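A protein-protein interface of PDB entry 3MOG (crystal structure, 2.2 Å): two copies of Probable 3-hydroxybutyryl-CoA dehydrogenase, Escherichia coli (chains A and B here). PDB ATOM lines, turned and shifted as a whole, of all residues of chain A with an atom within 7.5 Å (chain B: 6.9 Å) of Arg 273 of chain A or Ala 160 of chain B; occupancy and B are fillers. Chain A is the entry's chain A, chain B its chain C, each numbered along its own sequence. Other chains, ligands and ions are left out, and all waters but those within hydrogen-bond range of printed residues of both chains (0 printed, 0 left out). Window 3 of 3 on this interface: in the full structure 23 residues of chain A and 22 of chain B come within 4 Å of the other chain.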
ATOM      1  N   THR A 234      -9.699   1.548  19.730  1.00  0.00           N
ATOM      2  CA  THR A 234      -9.081   0.298  20.203  1.00  0.00           C
ATOM      3  C   THR A 234     -10.089  -0.859  20.242  1.00  0.00           C
ATOM      4  O   THR A 234      -9.731  -1.990  19.915  1.00  0.00           O
ATOM      5  CB  THR A 234      -8.330   0.435  21.574  1.00  0.00           C
ATOM      6  OG1 THR A 234      -9.238   0.799  22.618  1.00  0.00           O
ATOM      7  CG2 THR A 234      -7.236   1.459  21.500  1.00  0.00           C
ATOM      8  N   ASP A 235     -11.338  -0.570  20.615  1.00  0.00           N
ATOM      9  CA  ASP A 235     -12.432  -1.559  20.527  1.00  0.00           C
ATOM     10  C   ASP A 235     -12.650  -2.076  19.100  1.00  0.00           C
ATOM     11  O   ASP A 235     -12.918  -3.252  18.902  1.00  0.00           O
ATOM     12  CB  ASP A 235     -13.755  -1.000  21.077  1.00  0.00           C
ATOM     13  CG  ASP A 235     -13.913  -1.217  22.582  1.00  0.00           C
ATOM     14  OD1 ASP A 235     -12.935  -1.649  23.231  1.00  0.00           O
ATOM     15  OD2 ASP A 235     -15.006  -0.932  23.124  1.00  0.00           O
ATOM     16  N   GLY A 238      -9.559  -4.076  17.976  1.00  0.00           N
ATOM     17  CA  GLY A 238      -9.414  -5.285  18.762  1.00  0.00           C
ATOM     18  C   GLY A 238      -8.399  -4.982  19.848  1.00  0.00           C
ATOM     19  O   GLY A 238      -7.278  -4.539  19.561  1.00  0.00           O
ATOM     20  N   GLN A 239      -8.787  -5.216  21.096  1.00  0.00           N
ATOM     21  CA  GLN A 239      -7.957  -4.854  22.225  1.00  0.00           C
ATOM     22  C   GLN A 239      -6.690  -5.658  22.243  1.00  0.00           C
ATOM     23  O   GLN A 239      -5.630  -5.126  22.558  1.00  0.00           O
ATOM     24  CB  GLN A 239      -8.716  -4.981  23.550  1.00  0.00           C
ATOM     25  CG  GLN A 239      -9.820  -3.916  23.740  1.00  0.00           C
ATOM     26  CD  GLN A 239      -9.302  -2.473  23.859  1.00  0.00           C
ATOM     27  OE1 GLN A 239      -8.100  -2.216  24.039  1.00  0.00           O
ATOM     28  NE2 GLN A 239     -10.219  -1.527  23.756  1.00  0.00           N
ATOM     29  N   ASP A 240      -6.797  -6.924  21.852  1.00  0.00           N
ATOM     30  CA  ASP A 240      -5.640  -7.790  21.755  1.00  0.00           C
ATOM     31  C   ASP A 240      -4.632  -7.332  20.697  1.00  0.00           C
ATOM     32  O   ASP A 240      -3.436  -7.318  20.970  1.00  0.00           O
ATOM     33  CB  ASP A 240      -6.061  -9.258  21.566  1.00  0.00           C
ATOM     34  CG  ASP A 240      -6.815  -9.517  20.257  1.00  0.00           C
ATOM     35  OD1 ASP A 240      -7.624  -8.676  19.801  1.00  0.00           O
ATOM     36  OD2 ASP A 240      -6.599 -10.607  19.693  1.00  0.00           O
ATOM     37  N   GLN A 265      -5.650  -1.710  29.857  1.00  0.00           N
ATOM     38  CA  GLN A 265      -5.807  -2.419  28.587  1.00  0.00           C
ATOM     39  C   GLN A 265      -5.471  -3.903  28.749  1.00  0.00           C
ATOM     40  O   GLN A 265      -6.199  -4.755  28.245  1.00  0.00           O
ATOM     41  CB  GLN A 265      -4.942  -1.797  27.477  1.00  0.00           C
ATOM     42  CG  GLN A 265      -5.217  -2.420  26.111  1.00  0.00           C
ATOM     43  CD  GLN A 265      -4.509  -1.766  24.962  1.00  0.00           C
ATOM     44  OE1 GLN A 265      -3.393  -1.272  25.098  1.00  0.00           O
ATOM     45  NE2 GLN A 265      -5.148  -1.792  23.786  1.00  0.00           N
ATOM     46  N   GLU A 267      -5.746  -5.808  31.479  1.00  0.00           N
ATOM     47  CA  GLU A 267      -6.903  -6.412  32.148  1.00  0.00           C
ATOM     48  C   GLU A 267      -8.046  -6.798  31.171  1.00  0.00           C
ATOM     49  O   GLU A 267      -8.638  -7.875  31.294  1.00  0.00           O
ATOM     50  CB  GLU A 267      -7.407  -5.450  33.227  1.00  0.00           C
ATOM     51  CG  GLU A 267      -8.476  -5.992  34.115  1.00  0.00           C
ATOM     52  CD  GLU A 267      -7.975  -6.392  35.494  1.00  0.00           C
ATOM     53  OE1 GLU A 267      -6.929  -7.088  35.603  1.00  0.00           O
ATOM     54  OE2 GLU A 267      -8.663  -6.028  36.474  1.00  0.00           O
ATOM     55  N   LEU A 268      -8.346  -5.933  30.202  1.00  0.00           N
ATOM     56  CA  LEU A 268      -9.369  -6.246  29.191  1.00  0.00           C
ATOM     57  C   LEU A 268      -8.953  -7.406  28.270  1.00  0.00           C
ATOM     58  O   LEU A 268      -9.764  -8.284  27.989  1.00  0.00           O
ATOM     59  CB  LEU A 268      -9.749  -5.005  28.364  1.00  0.00           C
ATOM     60  CG  LEU A 268     -10.414  -3.803  29.057  1.00  0.00           C
ATOM     61  CD1 LEU A 268     -10.454  -2.643  28.090  1.00  0.00           C
ATOM     62  CD2 LEU A 268     -11.813  -4.095  29.608  1.00  0.00           C
ATOM     63  N   VAL A 269      -7.691  -7.408  27.827  1.00  0.00           N
ATOM     64  CA  VAL A 269      -7.166  -8.466  26.941  1.00  0.00           C
ATOM     65  C   VAL A 269      -7.189  -9.818  27.632  1.00  0.00           C
ATOM     66  O   VAL A 269      -7.714 -10.798  27.104  1.00  0.00           O
ATOM     67  CB  VAL A 269      -5.751  -8.130  26.441  1.00  0.00           C
ATOM     68  CG1 VAL A 269      -5.086  -9.324  25.719  1.00  0.00           C
ATOM     69  CG2 VAL A 269      -5.804  -6.920  25.547  1.00  0.00           C
ATOM     70  N   ILE A 270      -6.657  -9.835  28.848  1.00  0.00           N
ATOM     71  CA  ILE A 270      -6.637 -11.003  29.709  1.00  0.00           C
ATOM     72  C   ILE A 270      -8.060 -11.472  30.068  1.00  0.00           C
ATOM     73  O   ILE A 270      -8.331 -12.674  30.138  1.00  0.00           O
ATOM     74  CB  ILE A 270      -5.741 -10.709  30.935  1.00  0.00           C
ATOM     75  CG1 ILE A 270      -4.303 -11.139  30.639  1.00  0.00           C
ATOM     76  CG2 ILE A 270      -6.249 -11.371  32.196  1.00  0.00           C
ATOM     77  CD1 ILE A 270      -3.272 -10.609  31.635  1.00  0.00           C
ATOM     78  N   GLY A 271      -8.973 -10.528  30.243  1.00  0.00           N
ATOM     79  CA  GLY A 271     -10.362 -10.855  30.540  1.00  0.00           C
ATOM     80  C   GLY A 271     -11.216 -11.113  29.307  1.00  0.00           C
ATOM     81  O   GLY A 271     -12.420 -11.283  29.419  1.00  0.00           O
ATOM     82  N   GLY A 272     -10.599 -11.119  28.129  1.00  0.00           N
ATOM     83  CA  GLY A 272     -11.291 -11.500  26.892  1.00  0.00           C
ATOM     84  C   GLY A 272     -12.318 -10.493  26.398  1.00  0.00           C
ATOM     85  O   GLY A 272     -13.194 -10.828  25.605  1.00  0.00           O
ATOM     86  N   ARG A 273     -12.213  -9.257  26.875  1.00  0.00           N
ATOM     87  CA  ARG A 273     -13.089  -8.195  26.438  1.00  0.00           C
ATOM     88  C   ARG A 273     -12.393  -7.420  25.344  1.00  0.00           C
ATOM     89  O   ARG A 273     -11.926  -6.293  25.548  1.00  0.00           O
ATOM     90  CB  ARG A 273     -13.446  -7.278  27.595  1.00  0.00           C
ATOM     91  CG  ARG A 273     -14.098  -7.998  28.738  1.00  0.00           C
ATOM     92  CD  ARG A 273     -14.664  -7.007  29.684  1.00  0.00           C
ATOM     93  NE  ARG A 273     -15.305  -7.699  30.790  1.00  0.00           N
ATOM     94  CZ  ARG A 273     -15.912  -7.097  31.804  1.00  0.00           C
ATOM     95  NH1 ARG A 273     -16.475  -7.826  32.751  1.00  0.00           N
ATOM     96  NH2 ARG A 273     -15.957  -5.772  31.872  1.00  0.00           N
ATOM     97  N   LEU A 274     -12.356  -8.031  24.169  1.00  0.00           N
ATOM     98  CA  LEU A 274     -11.496  -7.577  23.088  1.00  0.00           C
ATOM     99  C   LEU A 274     -12.100  -6.491  22.186  1.00  0.00           C
ATOM    100  O   LEU A 274     -11.504  -6.120  21.170  1.00  0.00           O
ATOM    101  CB  LEU A 274     -10.990  -8.785  22.276  1.00  0.00           C
ATOM    102  CG  LEU A 274     -10.390  -9.942  23.095  1.00  0.00           C
ATOM    103  CD1 LEU A 274     -10.022 -11.163  22.236  1.00  0.00           C
ATOM    104  CD2 LEU A 274      -9.182  -9.480  23.925  1.00  0.00           C
ATOM    105  N   GLY A 275     -13.256  -5.951  22.561  1.00  0.00           N
ATOM    106  CA  GLY A 275     -13.865  -4.866  21.770  1.00  0.00           C
ATOM    107  C   GLY A 275     -15.111  -5.262  21.003  1.00  0.00           C
ATOM    108  O   GLY A 275     -15.909  -6.084  21.482  1.00  0.00           O
ATOM    109  N   LYS A 276     -15.280  -4.684  19.812  1.00  0.00           N
ATOM    110  CA  LYS A 276     -16.493  -4.891  18.999  1.00  0.00           C
ATOM    111  C   LYS A 276     -16.669  -6.358  18.611  1.00  0.00           C
ATOM    112  O   LYS A 276     -17.774  -6.894  18.682  1.00  0.00           O
ATOM    113  CB  LYS A 276     -16.474  -4.001  17.749  1.00  0.00           C
ATOM    114  CG  LYS A 276     -17.778  -4.001  16.932  1.00  0.00           C
ATOM    115  CD  LYS A 276     -17.810  -2.832  15.948  1.00  0.00           C
ATOM    116  CE  LYS A 276     -18.773  -3.058  14.780  1.00  0.00           C
ATOM    117  NZ  LYS A 276     -18.123  -3.774  13.639  1.00  0.00           N
ATOM    118  N   LYS A 277     -15.554  -6.998  18.265  1.00  0.00           N
ATOM    119  CA  LYS A 277     -15.507  -8.374  17.769  1.00  0.00           C
ATOM    120  C   LYS A 277     -15.999  -9.443  18.747  1.00  0.00           C
ATOM    121  O   LYS A 277     -16.314 -10.557  18.331  1.00  0.00           O
ATOM    122  CB  LYS A 277     -14.083  -8.726  17.310  1.00  0.00           C
ATOM    123  CG  LYS A 277     -13.024  -8.607  18.410  1.00  0.00           C
ATOM    124  CD  LYS A 277     -11.896  -9.622  18.253  1.00  0.00           C
ATOM    125  CE  LYS A 277     -10.751  -9.090  17.399  1.00  0.00           C
ATOM    126  NZ  LYS A 277      -9.480  -9.820  17.695  1.00  0.00           N
ATOM    127  N   SER A 278     -16.040  -9.120  20.037  1.00  0.00           N
ATOM    128  CA  SER A 278     -16.556 -10.050  21.033  1.00  0.00           C
ATOM    129  C   SER A 278     -17.683  -9.426  21.866  1.00  0.00           C
ATOM    130  O   SER A 278     -18.090  -9.967  22.892  1.00  0.00           O
ATOM    131  CB  SER A 278     -15.423 -10.616  21.902  1.00  0.00           C
ATOM    132  OG  SER A 278     -14.838  -9.621  22.711  1.00  0.00           O
ATOM    133  N   GLY A 279     -18.196  -8.290  21.396  1.00  0.00           N
ATOM    134  CA  GLY A 279     -19.392  -7.676  21.975  1.00  0.00           C
ATOM    135  C   GLY A 279     -19.168  -6.675  23.094  1.00  0.00           C
ATOM    136  O   GLY A 279     -20.080  -5.901  23.433  1.00  0.00           O
ATOM    137  N   LEU A 280     -17.956  -6.682  23.658  1.00  0.00           N
ATOM    138  CA  LEU A 280     -17.610  -5.868  24.828  1.00  0.00           C
ATOM    139  C   LEU A 280     -16.091  -5.648  24.924  1.00  0.00           C
ATOM    140  O   LEU A 280     -15.307  -6.587  24.817  1.00  0.00           O
ATOM    141  CB  LEU A 280     -18.163  -6.532  26.095  1.00  0.00           C
ATOM    142  CG  LEU A 280     -17.777  -6.120  27.514  1.00  0.00           C
ATOM    143  CD1 LEU A 280     -18.374  -4.779  27.914  1.00  0.00           C
ATOM    144  CD2 LEU A 280     -18.226  -7.206  28.469  1.00  0.00           C
ATOM    145  N   GLY A 281     -15.691  -4.392  25.079  1.00  0.00           N
ATOM    146  CA  GLY A 281     -14.295  -4.039  25.325  1.00  0.00           C
ATOM    147  C   GLY A 281     -14.293  -2.946  26.361  1.00  0.00           C
ATOM    148  O   GLY A 281     -14.691  -3.180  27.499  1.00  0.00           O
ATOM    149  N   VAL A 282     -13.868  -1.747  25.956  1.00  0.00           N
ATOM    150  CA  VAL A 282     -14.106  -0.532  26.739  1.00  0.00           C
ATOM    151  C   VAL A 282     -15.619  -0.263  26.761  1.00  0.00           C
ATOM    152  O   VAL A 282     -16.187   0.143  27.776  1.00  0.00           O
ATOM    153  CB  VAL A 282     -13.366   0.692  26.127  1.00  0.00           C
ATOM    154  CG1 VAL A 282     -13.710   1.980  26.871  1.00  0.00           C
ATOM    155  CG2 VAL A 282     -11.861   0.475  26.129  1.00  0.00           C
ATOM    156  N   TYR A 283     -16.270  -0.513  25.629  1.00  0.00           N
ATOM    157  CA  TYR A 283     -17.680  -0.181  25.479  1.00  0.00           C
ATOM    158  C   TYR A 283     -18.533  -1.433  25.336  1.00  0.00           C
ATOM    159  O   TYR A 283     -18.036  -2.483  24.913  1.00  0.00           O
ATOM    160  CB  TYR A 283     -17.878   0.734  24.268  1.00  0.00           C
ATOM    161  CG  TYR A 283     -17.260   2.115  24.394  1.00  0.00           C
ATOM    162  CD1 TYR A 283     -16.180   2.490  23.594  1.00  0.00           C
ATOM    163  CD2 TYR A 283     -17.753   3.047  25.311  1.00  0.00           C
ATOM    164  CE1 TYR A 283     -15.612   3.761  23.694  1.00  0.00           C
ATOM    165  CE2 TYR A 283     -17.184   4.323  25.423  1.00  0.00           C
ATOM    166  CZ  TYR A 283     -16.115   4.668  24.605  1.00  0.00           C
ATOM    167  OH  TYR A 283     -15.540   5.920  24.692  1.00  0.00           O
ATOM    168  N   ARG A 286     -23.135  -4.614  22.548  1.00  0.00           N
ATOM    169  CA  ARG A 286     -24.394  -5.371  22.501  1.00  0.00           C
ATOM    170  C   ARG A 286     -25.607  -4.465  22.739  1.00  0.00           C
ATOM    171  O   ARG A 286     -26.746  -4.851  22.458  1.00  0.00           O
ATOM    172  CB  ARG A 286     -24.385  -6.502  23.537  1.00  0.00           C
ATOM    173  CG  ARG A 286     -23.189  -7.445  23.456  1.00  0.00           C
ATOM    174  CD  ARG A 286     -23.080  -8.325  24.700  1.00  0.00           C
ATOM    175  NE  ARG A 286     -22.737  -7.565  25.909  1.00  0.00           N
ATOM    176  CZ  ARG A 286     -22.682  -8.075  27.141  1.00  0.00           C
ATOM    177  NH1 ARG A 286     -22.360  -7.298  28.165  1.00  0.00           N
ATOM    178  NH2 ARG A 286     -22.946  -9.358  27.360  1.00  0.00           N
ATOM    179  N   THR B 126      -8.379 -11.699  37.334  1.00  0.00           N
ATOM    180  CA  THR B 126      -8.876 -11.585  35.968  1.00  0.00           C
ATOM    181  C   THR B 126      -8.424 -12.747  35.077  1.00  0.00           C
ATOM    182  O   THR B 126      -9.228 -13.284  34.322  1.00  0.00           O
ATOM    183  CB  THR B 126      -8.451 -10.229  35.359  1.00  0.00           C
ATOM    184  OG1 THR B 126      -8.786  -9.195  36.284  1.00  0.00           O
ATOM    185  CG2 THR B 126      -9.177  -9.960  34.047  1.00  0.00           C
ATOM    186  N   ALA B 129     -10.108 -15.927  36.316  1.00  0.00           N
ATOM    187  CA  ALA B 129     -11.540 -15.887  36.028  1.00  0.00           C
ATOM    188  C   ALA B 129     -11.863 -15.825  34.545  1.00  0.00           C
ATOM    189  O   ALA B 129     -13.045 -15.764  34.165  1.00  0.00           O
ATOM    190  CB  ALA B 129     -12.167 -14.697  36.720  1.00  0.00           C
ATOM    191  N   ASN B 134     -19.130 -18.615  35.320  1.00  0.00           N
ATOM    192  CA  ASN B 134     -19.750 -17.382  35.781  1.00  0.00           C
ATOM    193  C   ASN B 134     -18.682 -16.499  36.395  1.00  0.00           C
ATOM    194  O   ASN B 134     -18.492 -16.518  37.601  1.00  0.00           O
ATOM    195  CB  ASN B 134     -20.842 -17.679  36.805  1.00  0.00           C
ATOM    196  CG  ASN B 134     -22.131 -18.115  36.165  1.00  0.00           C
ATOM    197  OD1 ASN B 134     -22.191 -19.174  35.547  1.00  0.00           O
ATOM    198  ND2 ASN B 134     -23.178 -17.307  36.316  1.00  0.00           N
ATOM    199  N   PRO B 135     -17.977 -15.710  35.565  1.00  0.00           N
ATOM    200  CA  PRO B 135     -16.729 -15.083  36.029  1.00  0.00           C
ATOM    201  C   PRO B 135     -16.936 -14.090  37.179  1.00  0.00           C
ATOM    202  O   PRO B 135     -15.996 -13.785  37.914  1.00  0.00           O
ATOM    203  CB  PRO B 135     -16.210 -14.380  34.773  1.00  0.00           C
ATOM    204  CG  PRO B 135     -17.438 -14.091  33.971  1.00  0.00           C
ATOM    205  CD  PRO B 135     -18.401 -15.200  34.246  1.00  0.00           C
ATOM    206  N   GLU B 136     -18.180 -13.652  37.341  1.00  0.00           N
ATOM    207  CA  GLU B 136     -18.601 -12.667  38.327  1.00  0.00           C
ATOM    208  C   GLU B 136     -18.520 -13.125  39.779  1.00  0.00           C
ATOM    209  O   GLU B 136     -18.513 -12.292  40.693  1.00  0.00           O
ATOM    210  CB  GLU B 136     -20.040 -12.258  38.022  1.00  0.00           C
ATOM    211  CG  GLU B 136     -20.784 -13.297  37.177  1.00  0.00           C
ATOM    212  CD  GLU B 136     -22.192 -13.569  37.663  1.00  0.00           C
ATOM    213  OE1 GLU B 136     -22.891 -12.615  38.079  1.00  0.00           O
ATOM    214  OE2 GLU B 136     -22.599 -14.750  37.622  1.00  0.00           O
ATOM    215  N   ARG B 137     -18.501 -14.433  40.009  1.00  0.00           N
ATOM    216  CA  ARG B 137     -18.428 -14.933  41.380  1.00  0.00           C
ATOM    217  C   ARG B 137     -17.023 -15.403  41.725  1.00  0.00           C
ATOM    218  O   ARG B 137     -16.810 -16.032  42.753  1.00  0.00           O
ATOM    219  CB  ARG B 137     -19.500 -16.004  41.690  1.00  0.00           C
ATOM    220  CG  ARG B 137     -19.738 -17.064  40.611  1.00  0.00           C
ATOM    221  CD  ARG B 137     -18.575 -18.023  40.497  1.00  0.00           C
ATOM    222  NE  ARG B 137     -18.649 -18.858  39.304  1.00  0.00           N
ATOM    223  CZ  ARG B 137     -19.098 -20.109  39.294  1.00  0.00           C
ATOM    224  NH1 ARG B 137     -19.519 -20.679  40.420  1.00  0.00           N
ATOM    225  NH2 ARG B 137     -19.116 -20.790  38.156  1.00  0.00           N
ATOM    226  N   VAL B 138     -16.078 -15.116  40.833  1.00  0.00           N
ATOM    227  CA  VAL B 138     -14.661 -15.309  41.114  1.00  0.00           C
ATOM    228  C   VAL B 138     -14.106 -14.020  41.734  1.00  0.00           C
ATOM    229  O   VAL B 138     -14.438 -12.923  41.290  1.00  0.00           O
ATOM    230  CB  VAL B 138     -13.866 -15.688  39.851  1.00  0.00           C
ATOM    231  CG1 VAL B 138     -12.470 -16.169  40.206  1.00  0.00           C
ATOM    232  CG2 VAL B 138     -14.595 -16.760  39.059  1.00  0.00           C
ATOM    233  N   SER B 157     -11.139  -7.704  43.718  1.00  0.00           N
ATOM    234  CA  SER B 157     -11.973  -7.763  42.515  1.00  0.00           C
ATOM    235  C   SER B 157     -11.129  -7.942  41.259  1.00  0.00           C
ATOM    236  O   SER B 157     -10.180  -7.188  41.001  1.00  0.00           O
ATOM    237  CB  SER B 157     -12.845  -6.525  42.365  1.00  0.00           C
ATOM    238  OG  SER B 157     -13.753  -6.384  43.447  1.00  0.00           O
ATOM    239  N   GLY B 158     -11.480  -8.957  40.477  1.00  0.00           N
ATOM    240  CA  GLY B 158     -11.032  -9.029  39.098  1.00  0.00           C
ATOM    241  C   GLY B 158     -11.937  -8.138  38.278  1.00  0.00           C
ATOM    242  O   GLY B 158     -12.912  -7.567  38.797  1.00  0.00           O
ATOM    243  N   LEU B 159     -11.627  -8.036  36.990  1.00  0.00           N
ATOM    244  CA  LEU B 159     -12.417  -7.239  36.049  1.00  0.00           C
ATOM    245  C   LEU B 159     -13.915  -7.532  36.112  1.00  0.00           C
ATOM    246  O   LEU B 159     -14.727  -6.608  36.179  1.00  0.00           O
ATOM    247  CB  LEU B 159     -11.894  -7.475  34.626  1.00  0.00           C
ATOM    248  CG  LEU B 159     -12.496  -6.723  33.444  1.00  0.00           C
ATOM    249  CD1 LEU B 159     -12.104  -5.244  33.510  1.00  0.00           C
ATOM    250  CD2 LEU B 159     -12.020  -7.379  32.159  1.00  0.00           C
ATOM    251  N   ALA B 160     -14.253  -8.824  36.127  1.00  0.00           N
ATOM    252  CA  ALA B 160     -15.634  -9.304  36.069  1.00  0.00           C
ATOM    253  C   ALA B 160     -16.350  -9.380  37.416  1.00  0.00           C
ATOM    254  O   ALA B 160     -17.576  -9.491  37.447  1.00  0.00           O
ATOM    255  CB  ALA B 160     -15.680 -10.674  35.379  1.00  0.00           C
ATOM    256  N   THR B 161     -15.589  -9.323  38.511  1.00  0.00           N
ATOM    257  CA  THR B 161     -16.120  -9.550  39.867  1.00  0.00           C
ATOM    258  C   THR B 161     -17.284  -8.634  40.212  1.00  0.00           C
ATOM    259  O   THR B 161     -17.127  -7.408  40.255  1.00  0.00           O
ATOM    260  CB  THR B 161     -15.027  -9.362  40.953  1.00  0.00           C
ATOM    261  OG1 THR B 161     -13.927 -10.243  40.705  1.00  0.00           O
ATOM    262  CG2 THR B 161     -15.576  -9.628  42.362  1.00  0.00           C
ATOM    263  N   ALA B 162     -18.442  -9.238  40.478  1.00  0.00           N
ATOM    264  CA  ALA B 162     -19.632  -8.498  40.905  1.00  0.00           C
ATOM    265  C   ALA B 162     -19.446  -7.831  42.267  1.00  0.00           C
ATOM    266  O   ALA B 162     -18.691  -8.318  43.119  1.00  0.00           O
ATOM    267  CB  ALA B 162     -20.856  -9.405  40.912  1.00  0.00           C
ATOM    268  N   ALA B 163     -20.136  -6.706  42.450  1.00  0.00           N
ATOM    269  CA  ALA B 163     -20.097  -5.940  43.691  1.00  0.00           C
ATOM    270  C   ALA B 163     -20.826  -6.612  44.857  1.00  0.00           C
ATOM    271  O   ALA B 163     -20.428  -6.420  46.018  1.00  0.00           O
ATOM    272  CB  ALA B 163     -20.634  -4.514  43.469  1.00  0.00           C
ATOM    273  N   HIS B 184      -8.598  -3.722  43.783  1.00  0.00           N
ATOM    274  CA  HIS B 184      -8.677  -4.324  42.459  1.00  0.00           C
ATOM    275  C   HIS B 184      -7.495  -5.254  42.270  1.00  0.00           C
ATOM    276  O   HIS B 184      -6.536  -5.213  43.048  1.00  0.00           O
ATOM    277  CB  HIS B 184      -8.684  -3.245  41.369  1.00  0.00           C
ATOM    278  CG  HIS B 184      -9.266  -3.707  40.069  1.00  0.00           C
ATOM    279  ND1 HIS B 184     -10.603  -4.004  39.915  1.00  0.00           N
ATOM    280  CD2 HIS B 184      -8.690  -3.929  38.862  1.00  0.00           C
ATOM    281  CE1 HIS B 184     -10.827  -4.389  38.670  1.00  0.00           C
ATOM    282  NE2 HIS B 184      -9.683  -4.350  38.010  1.00  0.00           N
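Ala 160 of chain B touches just one residue of chain A: Arg 273.
Printed residues of chain A within 4 Å of Leu 159 of chain B: Glu 267 (3.5 Å) and Arg 273 (3.6 Å).
Of the printed residues of chain B, Gly 271 of chain A touches Thr 126 (3.8 Å).
Printed residues of chain A within 4 Å of His 184 of chain B: Glu 267 (2.5 Å).
Of the printed residues of chain B, Ile 270 of chain A touches Thr 126.
Of the printed residues of chain A, Thr 126 of chain B touches Glu 267 (2.9 Å), Ile 270 (3.7 Å) and Gly 271 (3.8 Å).
The nearest residue of chain B that does not touch Arg 273 of chain A is Thr 161 of chain B (6.0 Å).
The nearest printed residue of chain B that does not touch Gly 271 of chain A is Leu 159 of chain B (4.2 Å).
The backbone carbonyl oxygen (O) of Ser 157 of chain B sits at hydrogen-bond distance from a ring nitrogen (ND1) of His 184 of chain B (3.4 Å).
The backbone carbonyl oxygen (O) of Leu 268 of chain A is in hydrogen-bond range of the backbone NH (N) of Arg 273 of chain A.
The backbone NH of Leu 159 of chain B lies within hydrogen-bond range of the side-chain hydroxyl of Thr 126 of chain B, 3.1 Å away.
Among the printed residues, pairs that only touch across the chains: Glu 267 of chain A with Leu 159 of chain B, Arg 273 of chain A with Leu 159 of chain B, Arg 273 of chain A with Ala 160 of chain B, Ile 270 of chain A with Thr 126 of chain B and Gly 271 of chain A with Thr 126 of chain B.
OE2 of Glu 267 of chain A lies within hydrogen-bond range of NE2 of His 184 of chain B.
The side-chain carboxylate (OE1) of Glu 267 of chain A sits at hydrogen-bond distance from the side-chain hydroxyl (OG1) of Thr 126 of chain B.
No position is printed for both chains.
Of the 7 pairs that touch across the chains among the printed residues, none has its exchanged pair printed and touching as well.
Of the 15 printed residues of chain B, 4 touch a printed residue of chain A.
Printed residues of chain A that touch a printed residue of chain B: Glu 267, Ile 270, Gly 271 and Arg 273.
Among the printed residues, 7 pairs touch across the chains.
Among the printed residues, no Asp or Glu carboxylate lies within 4 Å of a Lys or Arg side-chain nitrogen of the other chain.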
